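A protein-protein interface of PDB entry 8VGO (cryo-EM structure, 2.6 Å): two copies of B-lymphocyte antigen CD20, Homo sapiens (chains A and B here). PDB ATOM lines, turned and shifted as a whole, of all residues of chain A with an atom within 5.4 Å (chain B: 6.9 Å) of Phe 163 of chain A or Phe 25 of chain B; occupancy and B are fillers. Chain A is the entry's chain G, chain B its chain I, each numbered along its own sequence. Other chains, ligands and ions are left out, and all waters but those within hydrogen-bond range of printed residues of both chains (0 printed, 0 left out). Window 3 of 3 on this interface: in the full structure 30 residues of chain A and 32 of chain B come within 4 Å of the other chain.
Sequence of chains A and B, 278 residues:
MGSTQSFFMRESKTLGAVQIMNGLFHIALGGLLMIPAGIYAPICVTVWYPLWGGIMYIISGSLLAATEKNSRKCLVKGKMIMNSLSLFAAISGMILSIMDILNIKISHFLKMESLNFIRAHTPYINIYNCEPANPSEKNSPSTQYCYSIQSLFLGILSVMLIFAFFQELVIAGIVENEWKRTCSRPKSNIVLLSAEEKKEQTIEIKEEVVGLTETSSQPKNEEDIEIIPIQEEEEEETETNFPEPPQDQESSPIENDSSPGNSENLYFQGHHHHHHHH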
ATOM      1  N   MET A  21      33.137 -27.905  -4.694  1.00  0.00           N
ATOM      2  CA  MET A  21      31.681 -27.839  -4.765  1.00  0.00           C
ATOM      3  C   MET A  21      31.195 -26.970  -5.921  1.00  0.00           C
ATOM      4  O   MET A  21      30.255 -27.345  -6.630  1.00  0.00           O
ATOM      5  CB  MET A  21      31.122 -27.331  -3.438  1.00  0.00           C
ATOM      6  CG  MET A  21      31.377 -28.269  -2.274  1.00  0.00           C
ATOM      7  SD  MET A  21      30.605 -29.877  -2.509  1.00  0.00           S
ATOM      8  CE  MET A  21      28.895 -29.468  -2.193  1.00  0.00           C
ATOM      9  N   ASN A  22      31.809 -25.800  -6.124  1.00  0.00           N
ATOM     10  CA  ASN A  22      31.495 -25.003  -7.308  1.00  0.00           C
ATOM     11  C   ASN A  22      31.761 -25.758  -8.604  1.00  0.00           C
ATOM     12  O   ASN A  22      31.057 -25.548  -9.598  1.00  0.00           O
ATOM     13  CB  ASN A  22      32.296 -23.701  -7.299  1.00  0.00           C
ATOM     14  CG  ASN A  22      31.718 -22.666  -6.359  1.00  0.00           C
ATOM     15  OD1 ASN A  22      30.516 -22.647  -6.104  1.00  0.00           O
ATOM     16  ND2 ASN A  22      32.574 -21.793  -5.844  1.00  0.00           N
ATOM     17  N   PHE A  25      28.781 -28.488  -8.993  1.00  0.00           N
ATOM     18  CA  PHE A  25      27.511 -27.857  -9.337  1.00  0.00           C
ATOM     19  C   PHE A  25      27.506 -27.267 -10.741  1.00  0.00           C
ATOM     20  O   PHE A  25      26.459 -27.254 -11.394  1.00  0.00           O
ATOM     21  CB  PHE A  25      27.166 -26.781  -8.312  1.00  0.00           C
ATOM     22  CG  PHE A  25      25.707 -26.434  -8.272  1.00  0.00           C
ATOM     23  CD1 PHE A  25      24.766 -27.400  -7.963  1.00  0.00           C
ATOM     24  CD2 PHE A  25      25.276 -25.147  -8.532  1.00  0.00           C
ATOM     25  CE1 PHE A  25      23.423 -27.092  -7.923  1.00  0.00           C
ATOM     26  CE2 PHE A  25      23.933 -24.834  -8.491  1.00  0.00           C
ATOM     27  CZ  PHE A  25      23.006 -25.807  -8.185  1.00  0.00           C
ATOM     28  N   HIS A  26      28.647 -26.775 -11.228  1.00  0.00           N
ATOM     29  CA  HIS A  26      28.743 -26.431 -12.644  1.00  0.00           C
ATOM     30  C   HIS A  26      28.508 -27.642 -13.537  1.00  0.00           C
ATOM     31  O   HIS A  26      27.787 -27.553 -14.536  1.00  0.00           O
ATOM     32  CB  HIS A  26      30.101 -25.801 -12.946  1.00  0.00           C
ATOM     33  CG  HIS A  26      30.146 -24.325 -12.712  1.00  0.00           C
ATOM     34  ND1 HIS A  26      30.302 -23.773 -11.459  1.00  0.00           N
ATOM     35  CD2 HIS A  26      30.051 -23.284 -13.572  1.00  0.00           C
ATOM     36  CE1 HIS A  26      30.304 -22.456 -11.558  1.00  0.00           C
ATOM     37  NE2 HIS A  26      30.153 -22.134 -12.829  1.00  0.00           N
ATOM     38  N   LEU A  29      24.754 -28.384 -13.339  1.00  0.00           N
ATOM     39  CA  LEU A  29      24.055 -27.401 -14.163  1.00  0.00           C
ATOM     40  C   LEU A  29      24.342 -27.583 -15.646  1.00  0.00           C
ATOM     41  O   LEU A  29      23.459 -27.346 -16.476  1.00  0.00           O
ATOM     42  CB  LEU A  29      24.424 -25.981 -13.735  1.00  0.00           C
ATOM     43  CG  LEU A  29      23.956 -25.519 -12.355  1.00  0.00           C
ATOM     44  CD1 LEU A  29      24.668 -24.238 -11.963  1.00  0.00           C
ATOM     45  CD2 LEU A  29      22.451 -25.329 -12.338  1.00  0.00           C
ATOM     46  N   SER A 158      21.584 -17.806 -15.077  1.00  0.00           N
ATOM     47  CA  SER A 158      21.850 -16.838 -14.015  1.00  0.00           C
ATOM     48  C   SER A 158      22.283 -17.507 -12.715  1.00  0.00           C
ATOM     49  O   SER A 158      23.025 -16.905 -11.932  1.00  0.00           O
ATOM     50  CB  SER A 158      20.613 -15.977 -13.776  1.00  0.00           C
ATOM     51  OG  SER A 158      19.490 -16.777 -13.455  1.00  0.00           O
ATOM     52  N   VAL A 159      21.832 -18.736 -12.462  1.00  0.00           N
ATOM     53  CA  VAL A 159      22.380 -19.524 -11.361  1.00  0.00           C
ATOM     54  C   VAL A 159      23.829 -19.912 -11.636  1.00  0.00           C
ATOM     55  O   VAL A 159      24.692 -19.814 -10.758  1.00  0.00           O
ATOM     56  CB  VAL A 159      21.505 -20.762 -11.100  1.00  0.00           C
ATOM     57  CG1 VAL A 159      22.227 -21.744 -10.195  1.00  0.00           C
ATOM     58  CG2 VAL A 159      20.184 -20.350 -10.479  1.00  0.00           C
ATOM     59  N   MET A 160      24.119 -20.363 -12.856  1.00  0.00           N
ATOM     60  CA  MET A 160      25.498 -20.664 -13.226  1.00  0.00           C
ATOM     61  C   MET A 160      26.391 -19.429 -13.179  1.00  0.00           C
ATOM     62  O   MET A 160      27.566 -19.520 -12.807  1.00  0.00           O
ATOM     63  CB  MET A 160      25.537 -21.297 -14.616  1.00  0.00           C
ATOM     64  CG  MET A 160      26.915 -21.765 -15.041  1.00  0.00           C
ATOM     65  SD  MET A 160      26.848 -23.038 -16.313  1.00  0.00           S
ATOM     66  CE  MET A 160      25.959 -22.173 -17.599  1.00  0.00           C
ATOM     67  N   LEU A 161      25.855 -18.265 -13.549  1.00  0.00           N
ATOM     68  CA  LEU A 161      26.630 -17.029 -13.470  1.00  0.00           C
ATOM     69  C   LEU A 161      27.018 -16.687 -12.034  1.00  0.00           C
ATOM     70  O   LEU A 161      28.185 -16.396 -11.750  1.00  0.00           O
ATOM     71  CB  LEU A 161      25.836 -15.886 -14.106  1.00  0.00           C
ATOM     72  CG  LEU A 161      26.457 -14.512 -14.394  1.00  0.00           C
ATOM     73  CD1 LEU A 161      25.510 -13.728 -15.276  1.00  0.00           C
ATOM     74  CD2 LEU A 161      26.768 -13.698 -13.144  1.00  0.00           C
ATOM     75  N   ILE A 162      26.053 -16.708 -11.114  1.00  0.00           N
ATOM     76  CA  ILE A 162      26.339 -16.294  -9.742  1.00  0.00           C
ATOM     77  C   ILE A 162      27.312 -17.242  -9.043  1.00  0.00           C
ATOM     78  O   ILE A 162      28.073 -16.816  -8.166  1.00  0.00           O
ATOM     79  CB  ILE A 162      25.024 -16.136  -8.953  1.00  0.00           C
ATOM     80  CG1 ILE A 162      25.281 -15.464  -7.604  1.00  0.00           C
ATOM     81  CG2 ILE A 162      24.342 -17.470  -8.747  1.00  0.00           C
ATOM     82  CD1 ILE A 162      24.033 -14.907  -6.957  1.00  0.00           C
ATOM     83  N   PHE A 163      27.317 -18.524  -9.407  1.00  0.00           N
ATOM     84  CA  PHE A 163      28.374 -19.423  -8.947  1.00  0.00           C
ATOM     85  C   PHE A 163      29.682 -19.266  -9.714  1.00  0.00           C
ATOM     86  O   PHE A 163      30.754 -19.465  -9.135  1.00  0.00           O
ATOM     87  CB  PHE A 163      27.884 -20.869  -9.005  1.00  0.00           C
ATOM     88  CG  PHE A 163      26.884 -21.198  -7.938  1.00  0.00           C
ATOM     89  CD1 PHE A 163      27.268 -21.249  -6.611  1.00  0.00           C
ATOM     90  CD2 PHE A 163      25.561 -21.435  -8.255  1.00  0.00           C
ATOM     91  CE1 PHE A 163      26.354 -21.540  -5.622  1.00  0.00           C
ATOM     92  CE2 PHE A 163      24.642 -21.725  -7.270  1.00  0.00           C
ATOM     93  CZ  PHE A 163      25.039 -21.779  -5.953  1.00  0.00           C
ATOM     94  N   ALA A 164      29.628 -18.915 -11.000  1.00  0.00           N
ATOM     95  CA  ALA A 164      30.847 -18.538 -11.712  1.00  0.00           C
ATOM     96  C   ALA A 164      31.477 -17.286 -11.113  1.00  0.00           C
ATOM     97  O   ALA A 164      32.707 -17.183 -11.020  1.00  0.00           O
ATOM     98  CB  ALA A 164      30.548 -18.330 -13.195  1.00  0.00           C
ATOM     99  N   PHE A 165      30.653 -16.324 -10.705  1.00  0.00           N
ATOM    100  CA  PHE A 165      31.151 -15.152  -9.995  1.00  0.00           C
ATOM    101  C   PHE A 165      31.725 -15.531  -8.633  1.00  0.00           C
ATOM    102  O   PHE A 165      32.710 -14.938  -8.180  1.00  0.00           O
ATOM    103  CB  PHE A 165      30.020 -14.134  -9.854  1.00  0.00           C
ATOM    104  CG  PHE A 165      30.378 -12.920  -9.052  1.00  0.00           C
ATOM    105  CD1 PHE A 165      31.411 -12.091  -9.448  1.00  0.00           C
ATOM    106  CD2 PHE A 165      29.661 -12.592  -7.914  1.00  0.00           C
ATOM    107  CE1 PHE A 165      31.732 -10.964  -8.718  1.00  0.00           C
ATOM    108  CE2 PHE A 165      29.979 -11.468  -7.178  1.00  0.00           C
ATOM    109  CZ  PHE A 165      31.014 -10.653  -7.583  1.00  0.00           C
ATOM    110  N   PHE A 166      31.110 -16.509  -7.964  1.00  0.00           N
ATOM    111  CA  PHE A 166      31.615 -16.998  -6.683  1.00  0.00           C
ATOM    112  C   PHE A 166      33.024 -17.571  -6.804  1.00  0.00           C
ATOM    113  O   PHE A 166      33.853 -17.388  -5.906  1.00  0.00           O
ATOM    114  CB  PHE A 166      30.655 -18.053  -6.130  1.00  0.00           C
ATOM    115  CG  PHE A 166      30.669 -18.180  -4.631  1.00  0.00           C
ATOM    116  CD1 PHE A 166      31.818 -18.566  -3.960  1.00  0.00           C
ATOM    117  CD2 PHE A 166      29.524 -17.930  -3.894  1.00  0.00           C
ATOM    118  CE1 PHE A 166      31.828 -18.689  -2.586  1.00  0.00           C
ATOM    119  CE2 PHE A 166      29.528 -18.051  -2.517  1.00  0.00           C
ATOM    120  CZ  PHE A 166      30.683 -18.432  -1.863  1.00  0.00           C
ATOM    121  N   GLN A 167      33.316 -18.261  -7.906  1.00  0.00           N
ATOM    122  CA  GLN A 167      34.678 -18.728  -8.161  1.00  0.00           C
ATOM    123  C   GLN A 167      35.677 -17.582  -8.268  1.00  0.00           C
ATOM    124  O   GLN A 167      36.769 -17.647  -7.696  1.00  0.00           O
ATOM    125  CB  GLN A 167      34.716 -19.584  -9.425  1.00  0.00           C
ATOM    126  CG  GLN A 167      34.399 -21.034  -9.162  1.00  0.00           C
ATOM    127  CD  GLN A 167      35.417 -21.665  -8.236  1.00  0.00           C
ATOM    128  OE1 GLN A 167      35.195 -21.768  -7.031  1.00  0.00           O
ATOM    129  NE2 GLN A 167      36.549 -22.073  -8.792  1.00  0.00           N
ATOM    130  N   VAL B  18      31.385 -27.750   2.799  1.00  0.00           N
ATOM    131  CA  VAL B  18      30.571 -28.633   1.963  1.00  0.00           C
ATOM    132  C   VAL B  18      29.090 -28.538   2.314  1.00  0.00           C
ATOM    133  O   VAL B  18      28.234 -28.482   1.424  1.00  0.00           O
ATOM    134  CB  VAL B  18      31.084 -30.080   2.078  1.00  0.00           C
ATOM    135  CG1 VAL B  18      30.119 -31.042   1.414  1.00  0.00           C
ATOM    136  CG2 VAL B  18      32.468 -30.200   1.470  1.00  0.00           C
ATOM    137  N   ILE B  20      27.518 -25.946   3.730  1.00  0.00           N
ATOM    138  CA  ILE B  20      27.059 -24.635   3.272  1.00  0.00           C
ATOM    139  C   ILE B  20      26.826 -24.628   1.765  1.00  0.00           C
ATOM    140  O   ILE B  20      25.795 -24.149   1.280  1.00  0.00           O
ATOM    141  CB  ILE B  20      28.056 -23.541   3.692  1.00  0.00           C
ATOM    142  CG1 ILE B  20      27.959 -23.283   5.194  1.00  0.00           C
ATOM    143  CG2 ILE B  20      27.808 -22.263   2.917  1.00  0.00           C
ATOM    144  CD1 ILE B  20      29.039 -22.379   5.722  1.00  0.00           C
ATOM    145  N   MET B  21      27.774 -25.169   1.001  1.00  0.00           N
ATOM    146  CA  MET B  21      27.611 -25.228  -0.448  1.00  0.00           C
ATOM    147  C   MET B  21      26.420 -26.088  -0.862  1.00  0.00           C
ATOM    148  O   MET B  21      25.669 -25.713  -1.770  1.00  0.00           O
ATOM    149  CB  MET B  21      28.895 -25.745  -1.090  1.00  0.00           C
ATOM    150  CG  MET B  21      30.104 -24.859  -0.842  1.00  0.00           C
ATOM    151  SD  MET B  21      29.855 -23.160  -1.381  1.00  0.00           S
ATOM    152  CE  MET B  21      29.623 -23.398  -3.136  1.00  0.00           C
ATOM    153  N   ASN B  22      26.230 -27.244  -0.221  1.00  0.00           N
ATOM    154  CA  ASN B  22      25.010 -28.018  -0.445  1.00  0.00           C
ATOM    155  C   ASN B  22      23.749 -27.229  -0.115  1.00  0.00           C
ATOM    156  O   ASN B  22      22.711 -27.427  -0.757  1.00  0.00           O
ATOM    157  CB  ASN B  22      25.039 -29.307   0.376  1.00  0.00           C
ATOM    158  CG  ASN B  22      25.881 -30.389  -0.263  1.00  0.00           C
ATOM    159  OD1 ASN B  22      25.979 -30.472  -1.485  1.00  0.00           O
ATOM    160  ND2 ASN B  22      26.487 -31.233   0.562  1.00  0.00           N
ATOM    161  N   GLY B  23      23.809 -26.344   0.878  1.00  0.00           N
ATOM    162  CA  GLY B  23      22.669 -25.485   1.159  1.00  0.00           C
ATOM    163  C   GLY B  23      22.365 -24.505   0.041  1.00  0.00           C
ATOM    164  O   GLY B  23      21.224 -24.395  -0.415  1.00  0.00           O
ATOM    165  N   LEU B  24      23.386 -23.777  -0.411  1.00  0.00           N
ATOM    166  CA  LEU B  24      23.219 -22.815  -1.497  1.00  0.00           C
ATOM    167  C   LEU B  24      22.772 -23.478  -2.795  1.00  0.00           C
ATOM    168  O   LEU B  24      21.931 -22.931  -3.517  1.00  0.00           O
ATOM    169  CB  LEU B  24      24.524 -22.050  -1.713  1.00  0.00           C
ATOM    170  CG  LEU B  24      25.010 -21.226  -0.520  1.00  0.00           C
ATOM    171  CD1 LEU B  24      26.342 -20.567  -0.829  1.00  0.00           C
ATOM    172  CD2 LEU B  24      23.973 -20.190  -0.124  1.00  0.00           C
ATOM    173  N   PHE B  25      23.320 -24.652  -3.111  1.00  0.00           N
ATOM    174  CA  PHE B  25      22.872 -25.386  -4.293  1.00  0.00           C
ATOM    175  C   PHE B  25      21.398 -25.766  -4.214  1.00  0.00           C
ATOM    176  O   PHE B  25      20.672 -25.654  -5.206  1.00  0.00           O
ATOM    177  CB  PHE B  25      23.717 -26.647  -4.485  1.00  0.00           C
ATOM    178  CG  PHE B  25      25.187 -26.386  -4.681  1.00  0.00           C
ATOM    179  CD1 PHE B  25      25.654 -25.125  -5.005  1.00  0.00           C
ATOM    180  CD2 PHE B  25      26.101 -27.415  -4.540  1.00  0.00           C
ATOM    181  CE1 PHE B  25      27.005 -24.899  -5.182  1.00  0.00           C
ATOM    182  CE2 PHE B  25      27.450 -27.192  -4.716  1.00  0.00           C
ATOM    183  CZ  PHE B  25      27.902 -25.933  -5.035  1.00  0.00           C
ATOM    184  N   HIS B  26      20.932 -26.213  -3.047  1.00  0.00           N
ATOM    185  CA  HIS B  26      19.507 -26.482  -2.876  1.00  0.00           C
ATOM    186  C   HIS B  26      18.661 -25.227  -3.061  1.00  0.00           C
ATOM    187  O   HIS B  26      17.626 -25.261  -3.735  1.00  0.00           O
ATOM    188  CB  HIS B  26      19.253 -27.108  -1.506  1.00  0.00           C
ATOM    189  CG  HIS B  26      19.468 -28.587  -1.474  1.00  0.00           C
ATOM    190  ND1 HIS B  26      20.720 -29.156  -1.384  1.00  0.00           N
ATOM    191  CD2 HIS B  26      18.591 -29.616  -1.529  1.00  0.00           C
ATOM    192  CE1 HIS B  26      20.604 -30.471  -1.380  1.00  0.00           C
ATOM    193  NE2 HIS B  26      19.323 -30.776  -1.467  1.00  0.00           N
ATOM    194  N   ILE B  27      19.080 -24.110  -2.467  1.00  0.00           N
ATOM    195  CA  ILE B  27      18.339 -22.860  -2.622  1.00  0.00           C
ATOM    196  C   ILE B  27      18.282 -22.435  -4.085  1.00  0.00           C
ATOM    197  O   ILE B  27      17.231 -22.016  -4.585  1.00  0.00           O
ATOM    198  CB  ILE B  27      18.955 -21.763  -1.736  1.00  0.00           C
ATOM    199  CG1 ILE B  27      18.821 -22.138  -0.260  1.00  0.00           C
ATOM    200  CG2 ILE B  27      18.285 -20.427  -1.996  1.00  0.00           C
ATOM    201  CD1 ILE B  27      19.782 -21.404   0.644  1.00  0.00           C
ATOM    202  N   ALA B  28      19.406 -22.539  -4.796  1.00  0.00           N
ATOM    203  CA  ALA B  28      19.428 -22.199  -6.216  1.00  0.00           C
ATOM    204  C   ALA B  28      18.556 -23.139  -7.041  1.00  0.00           C
ATOM    205  O   ALA B  28      17.774 -22.691  -7.887  1.00  0.00           O
ATOM    206  CB  ALA B  28      20.866 -22.213  -6.732  1.00  0.00           C
ATOM    207  N   LEU B  29      18.680 -24.448  -6.813  1.00  0.00           N
ATOM    208  CA  LEU B  29      17.796 -25.406  -7.476  1.00  0.00           C
ATOM    209  C   LEU B  29      16.336 -25.188  -7.101  1.00  0.00           C
ATOM    210  O   LEU B  29      15.443 -25.390  -7.930  1.00  0.00           O
ATOM    211  CB  LEU B  29      18.219 -26.838  -7.149  1.00  0.00           C
ATOM    212  CG  LEU B  29      19.568 -27.296  -7.699  1.00  0.00           C
ATOM    213  CD1 LEU B  29      20.005 -28.587  -7.027  1.00  0.00           C
ATOM    214  CD2 LEU B  29      19.499 -27.469  -9.204  1.00  0.00           C
ATOM    215  N   GLY B  30      16.069 -24.782  -5.861  1.00  0.00           N
ATOM    216  CA  GLY B  30      14.697 -24.483  -5.480  1.00  0.00           C
ATOM    217  C   GLY B  30      14.113 -23.300  -6.225  1.00  0.00           C
ATOM    218  O   GLY B  30      13.012 -23.384  -6.776  1.00  0.00           O
ATOM    219  N   GLY B  31      14.834 -22.179  -6.248  1.00  0.00           N
ATOM    220  CA  GLY B  31      14.367 -21.029  -7.007  1.00  0.00           C
ATOM    221  C   GLY B  31      14.208 -21.334  -8.484  1.00  0.00           C
ATOM    222  O   GLY B  31      13.266 -20.869  -9.129  1.00  0.00           O
ATOM    223  N   PRO B  50      13.757 -27.131  -0.583  1.00  0.00           N
ATOM    224  CA  PRO B  50      15.032 -26.471  -0.903  1.00  0.00           C
ATOM    225  C   PRO B  50      15.257 -25.171  -0.153  1.00  0.00           C
ATOM    226  O   PRO B  50      16.415 -24.789   0.059  1.00  0.00           O
ATOM    227  CB  PRO B  50      14.937 -26.236  -2.416  1.00  0.00           C
ATOM    228  CG  PRO B  50      13.494 -26.279  -2.728  1.00  0.00           C
ATOM    229  CD  PRO B  50      12.891 -27.238  -1.769  1.00  0.00           C
ATOM    230  N   GLY B  54      17.687 -26.096   2.559  1.00  0.00           N
ATOM    231  CA  GLY B  54      18.914 -25.411   2.183  1.00  0.00           C
ATOM    232  C   GLY B  54      19.516 -24.575   3.297  1.00  0.00           C
ATOM    233  O   GLY B  54      20.700 -24.703   3.615  1.00  0.00           O
ATOM    234  N   ILE B  58      23.006 -24.520   5.661  1.00  0.00           N
ATOM    235  CA  ILE B  58      23.786 -23.341   6.028  1.00  0.00           C
ATOM    236  C   ILE B  58      23.973 -23.261   7.537  1.00  0.00           C
ATOM    237  O   ILE B  58      25.051 -22.908   8.027  1.00  0.00           O
ATOM    238  CB  ILE B  58      23.115 -22.068   5.483  1.00  0.00           C
ATOM    239  CG1 ILE B  58      22.775 -22.226   4.003  1.00  0.00           C
ATOM    240  CG2 ILE B  58      24.019 -20.867   5.687  1.00  0.00           C
ATOM    241  CD1 ILE B  58      23.975 -22.416   3.131  1.00  0.00           C
ATOM    242  N   MET B 160      18.965 -32.421  -7.576  1.00  0.00           N
ATOM    243  CA  MET B 160      18.682 -32.134  -6.172  1.00  0.00           C
ATOM    244  C   MET B 160      18.768 -33.383  -5.301  1.00  0.00           C
ATOM    245  O   MET B 160      19.215 -33.315  -4.152  1.00  0.00           O
ATOM    246  CB  MET B 160      17.304 -31.487  -6.041  1.00  0.00           C
ATOM    247  CG  MET B 160      16.971 -31.030  -4.635  1.00  0.00           C
ATOM    248  SD  MET B 160      15.725 -29.730  -4.611  1.00  0.00           S
ATOM    249  CE  MET B 160      14.371 -30.558  -5.434  1.00  0.00           C
ATOM    250  N   PHE B 163      22.587 -34.360  -4.650  1.00  0.00           N
ATOM    251  CA  PHE B 163      23.115 -33.488  -3.605  1.00  0.00           C
ATOM    252  C   PHE B 163      22.436 -33.676  -2.252  1.00  0.00           C
ATOM    253  O   PHE B 163      23.091 -33.530  -1.217  1.00  0.00           O
ATOM    254  CB  PHE B 163      23.024 -32.030  -4.050  1.00  0.00           C
ATOM    255  CG  PHE B 163      24.024 -31.668  -5.107  1.00  0.00           C
ATOM    256  CD1 PHE B 163      25.377 -31.659  -4.818  1.00  0.00           C
ATOM    257  CD2 PHE B 163      23.617 -31.353  -6.389  1.00  0.00           C
ATOM    258  CE1 PHE B 163      26.303 -31.337  -5.785  1.00  0.00           C
ATOM    259  CE2 PHE B 163      24.540 -31.031  -7.360  1.00  0.00           C
ATOM    260  CZ  PHE B 163      25.884 -31.023  -7.058  1.00  0.00           C
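Among the printed residues, merely in contact across the chains: Met 21 of chain A with Asn 22 of chain B (3.2 Å), Met 21 of chain A with Phe 25 of chain B (3.2 Å), Asn 22 of chain A with Met 21 of chain B (3.2 Å), Phe 163 of chain A with Phe 25 of chain B (3.4 Å), Phe 25 of chain A with Phe 25 of chain B (3.5 Å), Met 21 of chain A with Met 21 of chain B (3.6 Å), Phe 25 of chain A with Phe 163 of chain B (3.7 Å), Val 159 of chain A with Ala 28 of chain B (3.8 Å), Phe 25 of chain A with Leu 29 of chain B (3.8 Å), Met 21 of chain A with Val 18 of chain B (3.8 Å) and Phe 163 of chain A with Ala 28 of chain B (3.8 Å).
O of Asn 22 of chain A is in hydrogen-bond range of ND1 of His 26 of chain A, at 2.7 Å. The side-chain amide nitrogen (ND2) of Asn 22 of chain A sits at hydrogen-bond distance from the side-chain amide oxygen (OE1) of Gln 167 of chain A. O of Val 18 of chain B lies within hydrogen-bond range of ND2 of Asn 22 of chain B (3.4 Å). The backbone carbonyl oxygen of Asn 22 of chain B is in hydrogen-bond range of a ring nitrogen (ND1) of His 26 of chain B (2.7 Å).
Of the 15 printed residues of chain A, 5 touch a printed residue of chain B. Printed residues of chain A that touch a printed residue of chain B: Met 21, Asn 22, Phe 25, Val 159 and Phe 163. Hydrophobic or aromatic side chains of chain A that line the printed part of chain B: Met 21, Phe 25, Val 159 and Phe 163. Along chain A the printed residues that touch a printed residue of chain B span positions 21 to 163. Hydrophobic or aromatic side chains of chain B within 4 Å of the printed part of chain A: Met 21, Phe 25, Ala 28, Leu 29 and Phe 163. Among the printed residues, 11 pairs touch across the chains. Among the printed residues, no Asp or Glu carboxylate lies within 4 Å of a Lys or Arg side-chain nitrogen of the other chain.
Of chain B, only Phe 25 (3.4 Å) and Ala 28 (3.8 Å) come within 4 Å of Phe 163 of chain A. Phe 25 of chain B touches just these residues of chain A: Met 21, Phe 25 and Phe 163. Of the printed residues of chain A, Leu 29 of chain B touches Phe 25. Printed residues of chain B within 4 Å of Asn 22 of chain A: Met 21. Printed residues of chain B within 4 Å of Met 21 of chain A: Val 18, Met 21, Asn 22 and Phe 25. The nearest residue of chain A that does not touch Phe 25 of chain B is Asn 22 of chain A (4.1 Å).
Met 21 of chain A touches its own counterpart, Met 21 of chain B. Met 21 of chain A touches Asn 22 of chain B, and with the chains exchanged Asn 22 of chain A touches Met 21 of chain B. Met 21 of chain A touches Phe 25 of chain B, but with the chains exchanged Phe 25 of chain A does not touch Met 21 of chain B (6.5 Å). Phe 25 of chain A touches its own counterpart, Phe 25 of chain B. Positions printed for both chains: 21, 22, 25, 26, 29, 160 and 163. Of the 11 pairs that touch across the chains among the printed residues, 6 have their exchanged pair printed and touching as well.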
